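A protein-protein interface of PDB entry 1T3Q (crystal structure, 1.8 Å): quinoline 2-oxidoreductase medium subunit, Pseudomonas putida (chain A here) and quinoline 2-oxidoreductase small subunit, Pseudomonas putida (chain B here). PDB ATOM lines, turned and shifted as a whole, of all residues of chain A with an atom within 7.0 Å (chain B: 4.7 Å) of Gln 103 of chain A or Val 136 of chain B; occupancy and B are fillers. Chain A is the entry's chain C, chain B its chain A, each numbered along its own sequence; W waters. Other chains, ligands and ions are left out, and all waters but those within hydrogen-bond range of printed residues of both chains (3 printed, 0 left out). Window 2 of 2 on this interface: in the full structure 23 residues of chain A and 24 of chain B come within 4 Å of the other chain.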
ATOM      1  N   PHE A  78      14.892  -8.469  20.970  1.00  0.00           N
ATOM      2  CA  PHE A  78      15.720  -7.512  20.245  1.00  0.00           C
ATOM      3  C   PHE A  78      16.458  -8.134  19.064  1.00  0.00           C
ATOM      4  O   PHE A  78      16.435  -7.592  17.959  1.00  0.00           O
ATOM      5  CB  PHE A  78      16.757  -6.871  21.170  1.00  0.00           C
ATOM      6  CG  PHE A  78      17.815  -6.105  20.430  1.00  0.00           C
ATOM      7  CD1 PHE A  78      17.524  -4.874  19.853  1.00  0.00           C
ATOM      8  CD2 PHE A  78      19.085  -6.648  20.251  1.00  0.00           C
ATOM      9  CE1 PHE A  78      18.482  -4.192  19.104  1.00  0.00           C
ATOM     10  CE2 PHE A  78      20.048  -5.975  19.504  1.00  0.00           C
ATOM     11  CZ  PHE A  78      19.745  -4.744  18.929  1.00  0.00           C
ATOM     12  N   VAL A 100       5.650  -5.888  20.868  1.00  0.00           N
ATOM     13  CA  VAL A 100       5.979  -6.457  22.170  1.00  0.00           C
ATOM     14  C   VAL A 100       6.704  -5.501  23.117  1.00  0.00           C
ATOM     15  O   VAL A 100       7.848  -5.107  22.873  1.00  0.00           O
ATOM     16  CB  VAL A 100       6.821  -7.746  22.006  1.00  0.00           C
ATOM     17  CG1 VAL A 100       7.262  -8.268  23.366  1.00  0.00           C
ATOM     18  CG2 VAL A 100       5.998  -8.804  21.279  1.00  0.00           C
ATOM     19  N   ALA A 101       6.019  -5.143  24.202  1.00  0.00           N
ATOM     20  CA  ALA A 101       6.556  -4.256  25.229  1.00  0.00           C
ATOM     21  C   ALA A 101       7.297  -3.046  24.663  1.00  0.00           C
ATOM     22  O   ALA A 101       6.859  -2.416  23.695  1.00  0.00           O
ATOM     23  CB  ALA A 101       7.483  -5.046  26.150  1.00  0.00           C
ATOM     24  N   HIS A 102       8.416  -2.719  25.294  1.00  0.00           N
ATOM     25  CA  HIS A 102       9.227  -1.600  24.857  1.00  0.00           C
ATOM     26  C   HIS A 102      10.673  -2.037  24.732  1.00  0.00           C
ATOM     27  O   HIS A 102      11.027  -3.166  25.077  1.00  0.00           O
ATOM     28  CB  HIS A 102       9.110  -0.430  25.840  1.00  0.00           C
ATOM     29  CG  HIS A 102       7.718   0.099  25.978  1.00  0.00           C
ATOM     30  ND1 HIS A 102       6.748  -0.544  26.717  1.00  0.00           N
ATOM     31  CD2 HIS A 102       7.117   1.181  25.429  1.00  0.00           C
ATOM     32  CE1 HIS A 102       5.609   0.119  26.615  1.00  0.00           C
ATOM     33  NE2 HIS A 102       5.806   1.169  25.839  1.00  0.00           N
ATOM     34  N   GLN A 103      11.497  -1.124  24.231  1.00  0.00           N
ATOM     35  CA  GLN A 103      12.918  -1.353  24.016  1.00  0.00           C
ATOM     36  C   GLN A 103      13.649  -2.097  25.135  1.00  0.00           C
ATOM     37  O   GLN A 103      14.216  -3.161  24.904  1.00  0.00           O
ATOM     38  CB  GLN A 103      13.599  -0.005  23.753  1.00  0.00           C
ATOM     39  CG  GLN A 103      15.103   0.015  23.953  1.00  0.00           C
ATOM     40  CD  GLN A 103      15.694   1.388  23.676  1.00  0.00           C
ATOM     41  OE1 GLN A 103      15.933   1.754  22.524  1.00  0.00           O
ATOM     42  NE2 GLN A 103      15.912   2.161  24.732  1.00  0.00           N
ATOM     43  N   ALA A 104      13.639  -1.526  26.337  1.00  0.00           N
ATOM     44  CA  ALA A 104      14.321  -2.111  27.488  1.00  0.00           C
ATOM     45  C   ALA A 104      13.915  -3.554  27.770  1.00  0.00           C
ATOM     46  O   ALA A 104      14.770  -4.408  27.998  1.00  0.00           O
ATOM     47  CB  ALA A 104      14.082  -1.251  28.727  1.00  0.00           C
ATOM     48  N   VAL A 105      12.614  -3.822  27.773  1.00  0.00           N
ATOM     49  CA  VAL A 105      12.130  -5.173  28.022  1.00  0.00           C
ATOM     50  C   VAL A 105      12.574  -6.095  26.889  1.00  0.00           C
ATOM     51  O   VAL A 105      13.014  -7.219  27.139  1.00  0.00           O
ATOM     52  CB  VAL A 105      10.585  -5.203  28.142  1.00  0.00           C
ATOM     53  CG1 VAL A 105      10.080  -6.637  28.143  1.00  0.00           C
ATOM     54  CG2 VAL A 105      10.160  -4.504  29.432  1.00  0.00           C
ATOM     55  N   ARG A 106      12.474  -5.612  25.652  1.00  0.00           N
ATOM     56  CA  ARG A 106      12.874  -6.415  24.493  1.00  0.00           C
ATOM     57  C   ARG A 106      14.363  -6.743  24.483  1.00  0.00           C
ATOM     58  O   ARG A 106      14.787  -7.697  23.832  1.00  0.00           O
ATOM     59  CB  ARG A 106      12.499  -5.716  23.177  1.00  0.00           C
ATOM     60  CG  ARG A 106      11.012  -5.758  22.848  1.00  0.00           C
ATOM     61  CD  ARG A 106      10.762  -5.500  21.367  1.00  0.00           C
ATOM     62  NE  ARG A 106      11.198  -4.170  20.951  1.00  0.00           N
ATOM     63  CZ  ARG A 106      10.470  -3.063  21.078  1.00  0.00           C
ATOM     64  NH1 ARG A 106       9.254  -3.110  21.608  1.00  0.00           N
ATOM     65  NH2 ARG A 106      10.965  -1.899  20.678  1.00  0.00           N
ATOM     66  N   ASN A 107      15.160  -5.958  25.202  1.00  0.00           N
ATOM     67  CA  ASN A 107      16.594  -6.216  25.253  1.00  0.00           C
ATOM     68  C   ASN A 107      16.918  -7.400  26.158  1.00  0.00           C
ATOM     69  O   ASN A 107      18.030  -7.915  26.122  1.00  0.00           O
ATOM     70  CB  ASN A 107      17.345  -4.977  25.745  1.00  0.00           C
ATOM     71  CG  ASN A 107      17.508  -3.923  24.661  1.00  0.00           C
ATOM     72  OD1 ASN A 107      17.744  -2.753  24.954  1.00  0.00           O
ATOM     73  ND2 ASN A 107      17.397  -4.339  23.404  1.00  0.00           N
ATOM     74  N   ARG A 108      15.951  -7.829  26.969  1.00  0.00           N
ATOM     75  CA  ARG A 108      16.165  -8.961  27.877  1.00  0.00           C
ATOM     76  C   ARG A 108      15.244 -10.146  27.606  1.00  0.00           C
ATOM     77  O   ARG A 108      15.653 -11.301  27.747  1.00  0.00           O
ATOM     78  CB  ARG A 108      15.985  -8.531  29.340  1.00  0.00           C
ATOM     79  CG  ARG A 108      17.082  -7.625  29.879  1.00  0.00           C
ATOM     80  CD  ARG A 108      17.038  -7.556  31.407  1.00  0.00           C
ATOM     81  NE  ARG A 108      17.360  -8.840  32.038  1.00  0.00           N
ATOM     82  CZ  ARG A 108      18.589  -9.343  32.148  1.00  0.00           C
ATOM     83  NH1 ARG A 108      18.777 -10.519  32.737  1.00  0.00           N
ATOM     84  NH2 ARG A 108      19.635  -8.666  31.685  1.00  0.00           N
ATOM     85  N   PRO B  64      19.822  -0.465  26.895  1.00  0.00           N
ATOM     86  CA  PRO B  64      18.956  -0.149  28.035  1.00  0.00           C
ATOM     87  C   PRO B  64      18.199  -1.375  28.552  1.00  0.00           C
ATOM     88  O   PRO B  64      17.644  -2.160  27.778  1.00  0.00           O
ATOM     89  CB  PRO B  64      18.031   0.936  27.477  1.00  0.00           C
ATOM     90  CG  PRO B  64      17.972   0.611  26.009  1.00  0.00           C
ATOM     91  CD  PRO B  64      19.402   0.265  25.686  1.00  0.00           C
ATOM     92  N   THR B 117      17.536   5.835  28.233  1.00  0.00           N
ATOM     93  CA  THR B 117      16.829   5.552  26.993  1.00  0.00           C
ATOM     94  C   THR B 117      17.224   6.555  25.907  1.00  0.00           C
ATOM     95  O   THR B 117      17.450   6.172  24.757  1.00  0.00           O
ATOM     96  CB  THR B 117      15.299   5.585  27.193  1.00  0.00           C
ATOM     97  OG1 THR B 117      14.928   4.605  28.172  1.00  0.00           O
ATOM     98  CG2 THR B 117      14.581   5.261  25.886  1.00  0.00           C
ATOM     99  N   SER B 120      20.555   5.748  24.305  1.00  0.00           N
ATOM    100  CA  SER B 120      20.410   4.618  23.396  1.00  0.00           C
ATOM    101  C   SER B 120      19.864   5.063  22.045  1.00  0.00           C
ATOM    102  O   SER B 120      20.344   4.630  21.000  1.00  0.00           O
ATOM    103  CB  SER B 120      19.477   3.571  24.002  1.00  0.00           C
ATOM    104  OG  SER B 120      19.310   2.483  23.110  1.00  0.00           O
ATOM    105  N   ILE B 121      18.850   5.923  22.077  1.00  0.00           N
ATOM    106  CA  ILE B 121      18.225   6.450  20.868  1.00  0.00           C
ATOM    107  C   ILE B 121      19.239   7.219  20.024  1.00  0.00           C
ATOM    108  O   ILE B 121      19.365   6.998  18.816  1.00  0.00           O
ATOM    109  CB  ILE B 121      17.076   7.428  21.218  1.00  0.00           C
ATOM    110  CG1 ILE B 121      15.935   6.678  21.904  1.00  0.00           C
ATOM    111  CG2 ILE B 121      16.589   8.136  19.962  1.00  0.00           C
ATOM    112  CD1 ILE B 121      14.823   7.583  22.405  1.00  0.00           C
ATOM    113  N   GLU B 132       9.751   9.701  16.457  1.00  0.00           N
ATOM    114  CA  GLU B 132      10.615   8.576  16.775  1.00  0.00           C
ATOM    115  C   GLU B 132      10.990   8.616  18.255  1.00  0.00           C
ATOM    116  O   GLU B 132      11.015   7.582  18.929  1.00  0.00           O
ATOM    117  CB  GLU B 132      11.873   8.617  15.891  1.00  0.00           C
ATOM    118  CG  GLU B 132      11.571   8.308  14.420  1.00  0.00           C
ATOM    119  CD  GLU B 132      12.713   8.637  13.459  1.00  0.00           C
ATOM    120  OE1 GLU B 132      12.602   8.254  12.274  1.00  0.00           O
ATOM    121  OE2 GLU B 132      13.706   9.278  13.869  1.00  0.00           O
ATOM    122  N   VAL B 133      11.275   9.811  18.761  1.00  0.00           N
ATOM    123  CA  VAL B 133      11.636   9.950  20.165  1.00  0.00           C
ATOM    124  C   VAL B 133      10.445   9.585  21.053  1.00  0.00           C
ATOM    125  O   VAL B 133      10.592   8.824  22.008  1.00  0.00           O
ATOM    126  CB  VAL B 133      12.114  11.381  20.493  1.00  0.00           C
ATOM    127  CG1 VAL B 133      12.435  11.496  21.981  1.00  0.00           C
ATOM    128  CG2 VAL B 133      13.366  11.712  19.675  1.00  0.00           C
ATOM    129  N   ARG B 134       9.266  10.111  20.737  1.00  0.00           N
ATOM    130  CA  ARG B 134       8.087   9.799  21.540  1.00  0.00           C
ATOM    131  C   ARG B 134       7.828   8.294  21.554  1.00  0.00           C
ATOM    132  O   ARG B 134       7.422   7.736  22.574  1.00  0.00           O
ATOM    133  CB  ARG B 134       6.857  10.549  21.014  1.00  0.00           C
ATOM    134  CG  ARG B 134       6.825  12.032  21.412  1.00  0.00           C
ATOM    135  CD  ARG B 134       5.609  12.748  20.831  1.00  0.00           C
ATOM    136  NE  ARG B 134       5.546  14.164  21.196  1.00  0.00           N
ATOM    137  CZ  ARG B 134       5.125  14.624  22.372  1.00  0.00           C
ATOM    138  NH1 ARG B 134       4.725  13.782  23.314  1.00  0.00           N
ATOM    139  NH2 ARG B 134       5.092  15.928  22.603  1.00  0.00           N
ATOM    140  N   GLU B 135       8.085   7.639  20.425  1.00  0.00           N
ATOM    141  CA  GLU B 135       7.888   6.200  20.301  1.00  0.00           C
ATOM    142  C   GLU B 135       8.836   5.408  21.185  1.00  0.00           C
ATOM    143  O   GLU B 135       8.413   4.529  21.937  1.00  0.00           O
ATOM    144  CB  GLU B 135       8.078   5.769  18.844  1.00  0.00           C
ATOM    145  CG  GLU B 135       7.022   6.322  17.911  1.00  0.00           C
ATOM    146  CD  GLU B 135       7.366   6.138  16.444  1.00  0.00           C
ATOM    147  OE1 GLU B 135       6.537   6.534  15.593  1.00  0.00           O
ATOM    148  OE2 GLU B 135       8.459   5.608  16.139  1.00  0.00           O
ATOM    149  N   VAL B 136      10.124   5.711  21.097  1.00  0.00           N
ATOM    150  CA  VAL B 136      11.105   4.993  21.896  1.00  0.00           C
ATOM    151  C   VAL B 136      11.044   5.357  23.378  1.00  0.00           C
ATOM    152  O   VAL B 136      11.313   4.518  24.237  1.00  0.00           O
ATOM    153  CB  VAL B 136      12.529   5.238  21.365  1.00  0.00           C
ATOM    154  CG1 VAL B 136      13.528   4.373  22.130  1.00  0.00           C
ATOM    155  CG2 VAL B 136      12.582   4.905  19.877  1.00  0.00           C
ATOM    156  N   MET B 137      10.672   6.599  23.683  1.00  0.00           N
ATOM    157  CA  MET B 137      10.594   7.040  25.076  1.00  0.00           C
ATOM    158  C   MET B 137       9.274   6.636  25.740  1.00  0.00           C
ATOM    159  O   MET B 137       9.081   6.885  26.930  1.00  0.00           O
ATOM    160  CB  MET B 137      10.749   8.565  25.163  1.00  0.00           C
ATOM    161  CG  MET B 137      12.072   9.139  24.631  1.00  0.00           C
ATOM    162  SD  MET B 137      13.553   8.553  25.485  1.00  0.00           S
ATOM    163  CE  MET B 137      13.269   9.185  27.171  1.00  0.00           C
ATOM    164  N   SER B 138       8.381   5.997  24.989  1.00  0.00           N
ATOM    165  CA  SER B 138       7.074   5.606  25.524  1.00  0.00           C
ATOM    166  C   SER B 138       7.135   4.616  26.683  1.00  0.00           C
ATOM    167  O   SER B 138       6.119   4.347  27.328  1.00  0.00           O
ATOM    168  CB  SER B 138       6.178   5.038  24.410  1.00  0.00           C
ATOM    169  OG  SER B 138       6.638   3.786  23.941  1.00  0.00           O
ATOM    170  N   GLY B 139       8.321   4.076  26.944  1.00  0.00           N
ATOM    171  CA  GLY B 139       8.491   3.135  28.035  1.00  0.00           C
ATOM    172  C   GLY B 139       9.048   3.786  29.291  1.00  0.00           C
ATOM    173  O   GLY B 139       9.382   3.100  30.259  1.00  0.00           O
HETATM  174  O   HOH W   1       4.874   2.397  28.792  1.00  0.00           O
HETATM  175  O   HOH W   2      10.539   1.589  23.594  1.00  0.00           O
HETATM  176  O   HOH W   3      14.751   1.863  27.130  1.00  0.00           O
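Gln 103 of chain A touches just these residues of chain B: Pro 64 (2.9 Å), Thr 117 (3.6 Å), Ser 120 (3.5 Å) and Val 136 (3.6 Å).
Of the printed residues of chain B, Ala 104 of chain A touches Pro 64 (3.3 Å).
Of the printed residues of chain A, Pro 64 of chain B touches Gln 103, Ala 104 and Asn 107.
Of the printed residues of chain A, Thr 117 of chain B touches Gln 103.
Printed residues of chain A within 4 Å of Ser 120 of chain B: Gln 103.
Of the printed residues of chain A, Gly 139 of chain B touches His 102 (3.5 Å).
The nearest residue of chain A that does not touch Val 136 of chain B is His 102 of chain A (5.5 Å).
The side-chain amide oxygen (OD1) of Asn 107 of chain A sits close to the backbone carbonyl oxygen (O) of Pro 64 of chain B.
NE2 of His 102 of chain A sits close to OG of Ser 138 of chain B, at 3.3 Å.
Among the printed residues, merely in contact across the chains: Gln 103 of chain A with Pro 64 of chain B (2.9 Å), Ala 104 of chain A with Pro 64 of chain B (3.3 Å), His 102 of chain A with Gly 139 of chain B (3.5 Å), Gln 103 of chain A with Ser 120 of chain B (3.5 Å), Gln 103 of chain A with Thr 117 of chain B (3.6 Å) and Gln 103 of chain A with Val 136 of chain B (3.6 Å).
Water W3 bridges NE2 of Gln 103 of chain A (2.7 Å) and OG1 of Thr 117 of chain B (2.9 Å).
Water W1 lies within hydrogen-bond range of the backbone carbonyl oxygen (O) of Ser 138 of chain B (2.7 Å) and a ring nitrogen (NE2) of His 102 of chain A (3.3 Å).
Water W2 bridges N of Gln 103 of chain A (2.9 Å) and O of Val 136 of chain B (3.1 Å).
O of Glu 135 of chain B lies within hydrogen-bond range of OG of Ser 138 of chain B, at 2.8 Å.
Of the 12 printed residues of chain B, 6 touch a printed residue of chain A.
Printed residues of chain B that touch a printed residue of chain A: Pro 64, Thr 117, Ser 120, Val 136, Ser 138 and Gly 139.
Hydrophobic or aromatic side chains of chain B within 4 Å of the printed part of chain A: Pro 64 and Val 136.
Hydrophobic or aromatic side chains of chain A that line the printed part of chain B: His 102 and Ala 104.
Along chain A the printed residues that touch a printed residue of chain B span positions 102 to 107.
Among the printed residues, no Asp or Glu carboxylate lies within 4 Å of a Lys or Arg side-chain nitrogen of the other chain.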
